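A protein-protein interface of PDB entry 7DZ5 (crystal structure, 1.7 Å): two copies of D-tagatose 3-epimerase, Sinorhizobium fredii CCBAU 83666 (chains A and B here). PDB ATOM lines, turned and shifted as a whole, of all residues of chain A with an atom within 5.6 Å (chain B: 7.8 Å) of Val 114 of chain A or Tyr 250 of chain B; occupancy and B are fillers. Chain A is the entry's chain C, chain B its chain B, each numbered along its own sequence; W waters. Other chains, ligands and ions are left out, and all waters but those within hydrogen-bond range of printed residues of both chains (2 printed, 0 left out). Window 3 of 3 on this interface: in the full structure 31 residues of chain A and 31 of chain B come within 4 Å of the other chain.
Val 114 of chain A touches two residues of chain B.
Of the printed residues of chain A, Tyr 250 of chain B touches Arg 111, Gly 113, Val 114 and Pro 115.
Of the printed residues of chain A, Gly 251 of chain B touches Arg 111.
Printed residues of chain B within 4 Å of Arg 111 of chain A: Tyr 250, Gly 251, Ala 253 and Trp 255.
Printed residues of chain B within 4 Å of Pro 116 of chain A: Trp 255 (3.9 Å).
Printed residues of chain A within 4 Å of Ala 253 of chain B: Arg 111 (3.8 Å).
Leu 252 of chain B touches none of the printed residues of chain A.
Pro 245 of chain B touches none of the printed residues of chain A.
The nearest printed residue of chain A that does not touch Tyr 250 of chain B is Thr 112 of chain A (7.5 Å).
The nearest printed residue of chain B that does not touch Pro 116 of chain A is Arg 256 of chain B (6.0 Å).
Water W2 lies within hydrogen-bond range of NH2 of Arg 111 of chain A (2.5 Å) and O of Gly 251 of chain B (2.9 Å).
Water W1 lies within hydrogen-bond range of the backbone carbonyl oxygen of Tyr 250 of chain B and the guanidinium group of Arg 111 of chain A.
O of Gly 251 of chain B is in hydrogen-bond range of NH2 of Arg 111 of chain A (3.3 Å).
Tyr 250 of chain B touches Arg 111 of chain A (O to NH2, 3.9 Å).
Arg 111 of chain A touches Ala 253 of chain B.
CZ2 of Trp 255 of chain B touches NE of Arg 111 of chain A, at 3.8 Å.
CB of Tyr 250 of chain B touches O of Gly 113 of chain A, at 3.1 Å.
Tyr 250 of chain B touches Val 114 of chain A.
Trp 255 of chain B touches Val 114 of chain A.
Tyr 250 of chain B touches Pro 115 of chain A (CE1 to CD, 3.4 Å).
O of Trp 255 of chain B touches CB of Pro 115 of chain A, at 3.6 Å.
Trp 255 of chain B touches Pro 116 of chain A.
CD1 of Trp 255 of chain B touches CA of His 153 of chain A, 3.6 Å away.
Of the 14 printed residues of chain B, 4 touch a printed residue of chain A.
Hydrophobic or aromatic side chains of chain B within 4 Å of the printed part of chain A: Tyr 250, Ala 253 and Trp 255.
Of the 8 printed residues of chain A, 6 touch a printed residue of chain B.
The backbone carbonyl oxygen of Val 114 of chain A is in hydrogen-bond range of the side-chain hydroxyl of Thr 112 of chain A, at 3.0 Å.
No position is printed for both chains.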
ATOM      1  N   ARG A 111      26.723 -35.081 -16.297  1.00  0.00           N
ATOM      2  CA  ARG A 111      25.892 -33.920 -16.563  1.00  0.00           C
ATOM      3  C   ARG A 111      24.642 -34.413 -17.294  1.00  0.00           C
ATOM      4  O   ARG A 111      24.773 -35.087 -18.316  1.00  0.00           O
ATOM      5  CB  ARG A 111      26.721 -32.984 -17.455  1.00  0.00           C
ATOM      6  CG  ARG A 111      26.302 -31.595 -17.587  1.00  0.00           C
ATOM      7  CD  ARG A 111      27.539 -30.702 -17.798  1.00  0.00           C
ATOM      8  NE  ARG A 111      27.130 -29.350 -18.114  1.00  0.00           N
ATOM      9  CZ  ARG A 111      27.923 -28.297 -18.137  1.00  0.00           C
ATOM     10  NH1 ARG A 111      29.222 -28.408 -17.855  1.00  0.00           N
ATOM     11  NH2 ARG A 111      27.404 -27.120 -18.447  1.00  0.00           N
ATOM     12  N   THR A 112      23.440 -34.101 -16.789  1.00  0.00           N
ATOM     13  CA  THR A 112      22.250 -34.302 -17.623  1.00  0.00           C
ATOM     14  C   THR A 112      21.928 -33.071 -18.452  1.00  0.00           C
ATOM     15  O   THR A 112      21.262 -33.179 -19.483  1.00  0.00           O
ATOM     16  CB  THR A 112      21.005 -34.629 -16.800  1.00  0.00           C
ATOM     17  OG1 THR A 112      20.773 -33.578 -15.855  1.00  0.00           O
ATOM     18  CG2 THR A 112      21.134 -35.976 -16.106  1.00  0.00           C
ATOM     19  N   GLY A 113      22.396 -31.909 -18.022  1.00  0.00           N
ATOM     20  CA  GLY A 113      22.005 -30.656 -18.606  1.00  0.00           C
ATOM     21  C   GLY A 113      20.929 -29.935 -17.831  1.00  0.00           C
ATOM     22  O   GLY A 113      20.654 -28.775 -18.131  1.00  0.00           O
ATOM     23  N   VAL A 114      20.317 -30.585 -16.847  1.00  0.00           N
ATOM     24  CA  VAL A 114      19.346 -29.934 -15.977  1.00  0.00           C
ATOM     25  C   VAL A 114      19.663 -30.251 -14.520  1.00  0.00           C
ATOM     26  O   VAL A 114      20.506 -31.115 -14.238  1.00  0.00           O
ATOM     27  CB  VAL A 114      17.910 -30.359 -16.322  1.00  0.00           C
ATOM     28  CG1 VAL A 114      17.546 -29.866 -17.708  1.00  0.00           C
ATOM     29  CG2 VAL A 114      17.756 -31.880 -16.186  1.00  0.00           C
ATOM     30  N   PRO A 115      19.037 -29.576 -13.568  1.00  0.00           N
ATOM     31  CA  PRO A 115      19.344 -29.836 -12.156  1.00  0.00           C
ATOM     32  C   PRO A 115      19.008 -31.260 -11.752  1.00  0.00           C
ATOM     33  O   PRO A 115      18.203 -31.941 -12.407  1.00  0.00           O
ATOM     34  CB  PRO A 115      18.457 -28.824 -11.415  1.00  0.00           C
ATOM     35  CG  PRO A 115      18.301 -27.700 -12.374  1.00  0.00           C
ATOM     36  CD  PRO A 115      18.170 -28.389 -13.718  1.00  0.00           C
ATOM     37  N   PRO A 116      19.611 -31.743 -10.671  1.00  0.00           N
ATOM     38  CA  PRO A 116      19.371 -33.121 -10.239  1.00  0.00           C
ATOM     39  C   PRO A 116      17.942 -33.320  -9.766  1.00  0.00           C
ATOM     40  O   PRO A 116      17.305 -32.400  -9.245  1.00  0.00           O
ATOM     41  CB  PRO A 116      20.373 -33.303  -9.093  1.00  0.00           C
ATOM     42  CG  PRO A 116      20.636 -31.910  -8.604  1.00  0.00           C
ATOM     43  CD  PRO A 116      20.614 -31.070  -9.818  1.00  0.00           C
ATOM     44  N   THR A 117      17.441 -34.541  -9.950  1.00  0.00           N
ATOM     45  CA  THR A 117      16.064 -34.872  -9.601  1.00  0.00           C
ATOM     46  C   THR A 117      16.000 -35.856  -8.438  1.00  0.00           C
ATOM     47  O   THR A 117      16.945 -36.591  -8.150  1.00  0.00           O
ATOM     48  CB  THR A 117      15.320 -35.467 -10.803  1.00  0.00           C
ATOM     49  OG1 THR A 117      15.855 -36.764 -11.103  1.00  0.00           O
ATOM     50  CG2 THR A 117      15.454 -34.571 -12.035  1.00  0.00           C
ATOM     51  N   HIS A 153      26.617 -33.196 -11.422  1.00  0.00           N
ATOM     52  CA  HIS A 153      25.498 -32.315 -11.113  1.00  0.00           C
ATOM     53  C   HIS A 153      24.752 -32.703  -9.843  1.00  0.00           C
ATOM     54  O   HIS A 153      23.799 -32.006  -9.469  1.00  0.00           O
ATOM     55  CB  HIS A 153      24.501 -32.283 -12.284  1.00  0.00           C
ATOM     56  CG  HIS A 153      23.815 -33.588 -12.526  1.00  0.00           C
ATOM     57  ND1 HIS A 153      24.506 -34.749 -12.810  1.00  0.00           N
ATOM     58  CD2 HIS A 153      22.501 -33.911 -12.551  1.00  0.00           C
ATOM     59  CE1 HIS A 153      23.641 -35.731 -12.991  1.00  0.00           C
ATOM     60  NE2 HIS A 153      22.420 -35.250 -12.844  1.00  0.00           N
ATOM     61  N   ILE B 108      31.025 -22.018 -25.120  1.00  0.00           N
ATOM     62  CA  ILE B 108      30.852 -22.769 -23.880  1.00  0.00           C
ATOM     63  C   ILE B 108      30.482 -24.201 -24.248  1.00  0.00           C
ATOM     64  O   ILE B 108      29.533 -24.439 -25.009  1.00  0.00           O
ATOM     65  CB  ILE B 108      29.775 -22.114 -22.995  1.00  0.00           C
ATOM     66  CG1 ILE B 108      30.055 -20.609 -22.811  1.00  0.00           C
ATOM     67  CG2 ILE B 108      29.668 -22.815 -21.655  1.00  0.00           C
ATOM     68  CD1 ILE B 108      31.373 -20.280 -22.114  1.00  0.00           C
ATOM     69  N   MET B 244      19.075 -15.723 -13.445  1.00  0.00           N
ATOM     70  CA  MET B 244      19.318 -16.052 -14.839  1.00  0.00           C
ATOM     71  C   MET B 244      18.195 -16.955 -15.346  1.00  0.00           C
ATOM     72  O   MET B 244      17.708 -17.820 -14.608  1.00  0.00           O
ATOM     73  CB  MET B 244      20.667 -16.745 -15.003  1.00  0.00           C
ATOM     74  CG  MET B 244      21.276 -16.562 -16.406  1.00  0.00           C
ATOM     75  SD  MET B 244      22.991 -17.087 -16.358  1.00  0.00           S
ATOM     76  CE  MET B 244      23.785 -15.547 -16.769  1.00  0.00           C
ATOM     77  N   PRO B 245      17.743 -16.769 -16.580  1.00  0.00           N
ATOM     78  CA  PRO B 245      16.758 -17.698 -17.165  1.00  0.00           C
ATOM     79  C   PRO B 245      17.253 -19.130 -17.098  1.00  0.00           C
ATOM     80  O   PRO B 245      18.417 -19.396 -17.424  1.00  0.00           O
ATOM     81  CB  PRO B 245      16.642 -17.217 -18.619  1.00  0.00           C
ATOM     82  CG  PRO B 245      17.052 -15.779 -18.575  1.00  0.00           C
ATOM     83  CD  PRO B 245      18.082 -15.658 -17.487  1.00  0.00           C
ATOM     84  N   PRO B 246      16.398 -20.088 -16.709  1.00  0.00           N
ATOM     85  CA  PRO B 246      16.916 -21.441 -16.412  1.00  0.00           C
ATOM     86  C   PRO B 246      17.709 -22.072 -17.544  1.00  0.00           C
ATOM     87  O   PRO B 246      18.783 -22.635 -17.302  1.00  0.00           O
ATOM     88  CB  PRO B 246      15.635 -22.236 -16.102  1.00  0.00           C
ATOM     89  CG  PRO B 246      14.690 -21.204 -15.567  1.00  0.00           C
ATOM     90  CD  PRO B 246      14.966 -19.963 -16.375  1.00  0.00           C
ATOM     91  N   GLU B 247      17.184 -22.008 -18.774  1.00  0.00           N
ATOM     92  CA  GLU B 247      17.879 -22.541 -19.947  1.00  0.00           C
ATOM     93  C   GLU B 247      19.330 -22.083 -19.998  1.00  0.00           C
ATOM     94  O   GLU B 247      20.253 -22.888 -20.206  1.00  0.00           O
ATOM     95  CB  GLU B 247      17.154 -22.097 -21.231  1.00  0.00           C
ATOM     96  CG  GLU B 247      15.625 -22.300 -21.268  1.00  0.00           C
ATOM     97  CD  GLU B 247      15.176 -23.490 -22.142  1.00  0.00           C
ATOM     98  OE1 GLU B 247      15.941 -24.471 -22.266  1.00  0.00           O
ATOM     99  OE2 GLU B 247      14.049 -23.451 -22.685  1.00  0.00           O
ATOM    100  N   VAL B 248      19.555 -20.777 -19.852  1.00  0.00           N
ATOM    101  CA  VAL B 248      20.918 -20.266 -19.914  1.00  0.00           C
ATOM    102  C   VAL B 248      21.705 -20.723 -18.683  1.00  0.00           C
ATOM    103  O   VAL B 248      22.857 -21.136 -18.790  1.00  0.00           O
ATOM    104  CB  VAL B 248      20.915 -18.732 -20.046  1.00  0.00           C
ATOM    105  CG1 VAL B 248      22.311 -18.223 -20.271  1.00  0.00           C
ATOM    106  CG2 VAL B 248      19.980 -18.275 -21.184  1.00  0.00           C
ATOM    107  N   ALA B 249      21.072 -20.668 -17.510  1.00  0.00           N
ATOM    108  CA  ALA B 249      21.749 -21.079 -16.282  1.00  0.00           C
ATOM    109  C   ALA B 249      22.212 -22.530 -16.356  1.00  0.00           C
ATOM    110  O   ALA B 249      23.323 -22.852 -15.933  1.00  0.00           O
ATOM    111  CB  ALA B 249      20.811 -20.881 -15.093  1.00  0.00           C
ATOM    112  N   TYR B 250      21.371 -23.429 -16.880  1.00  0.00           N
ATOM    113  CA  TYR B 250      21.777 -24.831 -16.951  1.00  0.00           C
ATOM    114  C   TYR B 250      23.012 -25.006 -17.841  1.00  0.00           C
ATOM    115  O   TYR B 250      23.878 -25.836 -17.546  1.00  0.00           O
ATOM    116  CB  TYR B 250      20.611 -25.703 -17.444  1.00  0.00           C
ATOM    117  CG  TYR B 250      19.353 -25.630 -16.617  1.00  0.00           C
ATOM    118  CD1 TYR B 250      19.361 -25.146 -15.320  1.00  0.00           C
ATOM    119  CD2 TYR B 250      18.135 -26.031 -17.146  1.00  0.00           C
ATOM    120  CE1 TYR B 250      18.191 -25.076 -14.567  1.00  0.00           C
ATOM    121  CE2 TYR B 250      16.974 -25.952 -16.410  1.00  0.00           C
ATOM    122  CZ  TYR B 250      17.002 -25.477 -15.126  1.00  0.00           C
ATOM    123  OH  TYR B 250      15.834 -25.400 -14.397  1.00  0.00           O
ATOM    124  N   GLY B 251      23.134 -24.212 -18.909  1.00  0.00           N
ATOM    125  CA  GLY B 251      24.301 -24.293 -19.776  1.00  0.00           C
ATOM    126  C   GLY B 251      25.591 -23.839 -19.133  1.00  0.00           C
ATOM    127  O   GLY B 251      26.673 -24.159 -19.641  1.00  0.00           O
ATOM    128  N   LEU B 252      25.499 -23.074 -18.049  1.00  0.00           N
ATOM    129  CA  LEU B 252      26.636 -22.606 -17.271  1.00  0.00           C
ATOM    130  C   LEU B 252      26.798 -23.399 -15.982  1.00  0.00           C
ATOM    131  O   LEU B 252      27.500 -22.962 -15.061  1.00  0.00           O
ATOM    132  CB  LEU B 252      26.464 -21.122 -16.984  1.00  0.00           C
ATOM    133  CG  LEU B 252      26.481 -20.291 -18.279  1.00  0.00           C
ATOM    134  CD1 LEU B 252      25.760 -18.982 -18.078  1.00  0.00           C
ATOM    135  CD2 LEU B 252      27.917 -20.067 -18.716  1.00  0.00           C
ATOM    136  N   ALA B 253      26.128 -24.541 -15.903  1.00  0.00           N
ATOM    137  CA  ALA B 253      26.281 -25.501 -14.817  1.00  0.00           C
ATOM    138  C   ALA B 253      25.763 -24.943 -13.495  1.00  0.00           C
ATOM    139  O   ALA B 253      26.310 -25.225 -12.429  1.00  0.00           O
ATOM    140  CB  ALA B 253      27.732 -25.963 -14.696  1.00  0.00           C
ATOM    141  N   VAL B 254      24.691 -24.157 -13.567  1.00  0.00           N
ATOM    142  CA  VAL B 254      23.976 -23.689 -12.386  1.00  0.00           C
ATOM    143  C   VAL B 254      22.886 -24.712 -12.079  1.00  0.00           C
ATOM    144  O   VAL B 254      21.826 -24.717 -12.711  1.00  0.00           O
ATOM    145  CB  VAL B 254      23.381 -22.295 -12.586  1.00  0.00           C
ATOM    146  CG1 VAL B 254      22.647 -21.872 -11.312  1.00  0.00           C
ATOM    147  CG2 VAL B 254      24.436 -21.294 -12.956  1.00  0.00           C
ATOM    148  N   TRP B 255      23.136 -25.556 -11.083  1.00  0.00           N
ATOM    149  CA  TRP B 255      22.263 -26.658 -10.715  1.00  0.00           C
ATOM    150  C   TRP B 255      21.448 -26.371  -9.468  1.00  0.00           C
ATOM    151  O   TRP B 255      20.678 -27.226  -9.033  1.00  0.00           O
ATOM    152  CB  TRP B 255      23.081 -27.924 -10.470  1.00  0.00           C
ATOM    153  CG  TRP B 255      24.093 -28.284 -11.512  1.00  0.00           C
ATOM    154  CD1 TRP B 255      25.381 -28.680 -11.297  1.00  0.00           C
ATOM    155  CD2 TRP B 255      23.888 -28.340 -12.930  1.00  0.00           C
ATOM    156  NE1 TRP B 255      25.994 -28.968 -12.493  1.00  0.00           N
ATOM    157  CE2 TRP B 255      25.103 -28.760 -13.509  1.00  0.00           C
ATOM    158  CE3 TRP B 255      22.795 -28.067 -13.764  1.00  0.00           C
ATOM    159  CZ2 TRP B 255      25.254 -28.913 -14.881  1.00  0.00           C
ATOM    160  CZ3 TRP B 255      22.940 -28.212 -15.101  1.00  0.00           C
ATOM    161  CH2 TRP B 255      24.159 -28.640 -15.662  1.00  0.00           C
ATOM    162  N   ARG B 256      21.630 -25.200  -8.877  1.00  0.00           N
ATOM    163  CA  ARG B 256      21.033 -24.807  -7.610  1.00  0.00           C
ATOM    164  C   ARG B 256      21.206 -23.298  -7.476  1.00  0.00           C
ATOM    165  O   ARG B 256      22.082 -22.711  -8.127  1.00  0.00           O
ATOM    166  CB  ARG B 256      21.702 -25.522  -6.425  1.00  0.00           C
ATOM    167  CG  ARG B 256      23.201 -25.208  -6.284  1.00  0.00           C
ATOM    168  CD  ARG B 256      23.894 -26.137  -5.300  1.00  0.00           C
ATOM    169  NE  ARG B 256      25.332 -25.879  -5.307  1.00  0.00           N
ATOM    170  CZ  ARG B 256      25.971 -25.063  -4.475  1.00  0.00           C
ATOM    171  NH1 ARG B 256      25.333 -24.431  -3.501  1.00  0.00           N
ATOM    172  NH2 ARG B 256      27.277 -24.897  -4.619  1.00  0.00           N
HETATM  173  O   HOH W   1      24.614 -28.045 -19.162  1.00  0.00           O
HETATM  174  O   HOH W   2      29.068 -25.286 -18.404  1.00  0.00           O
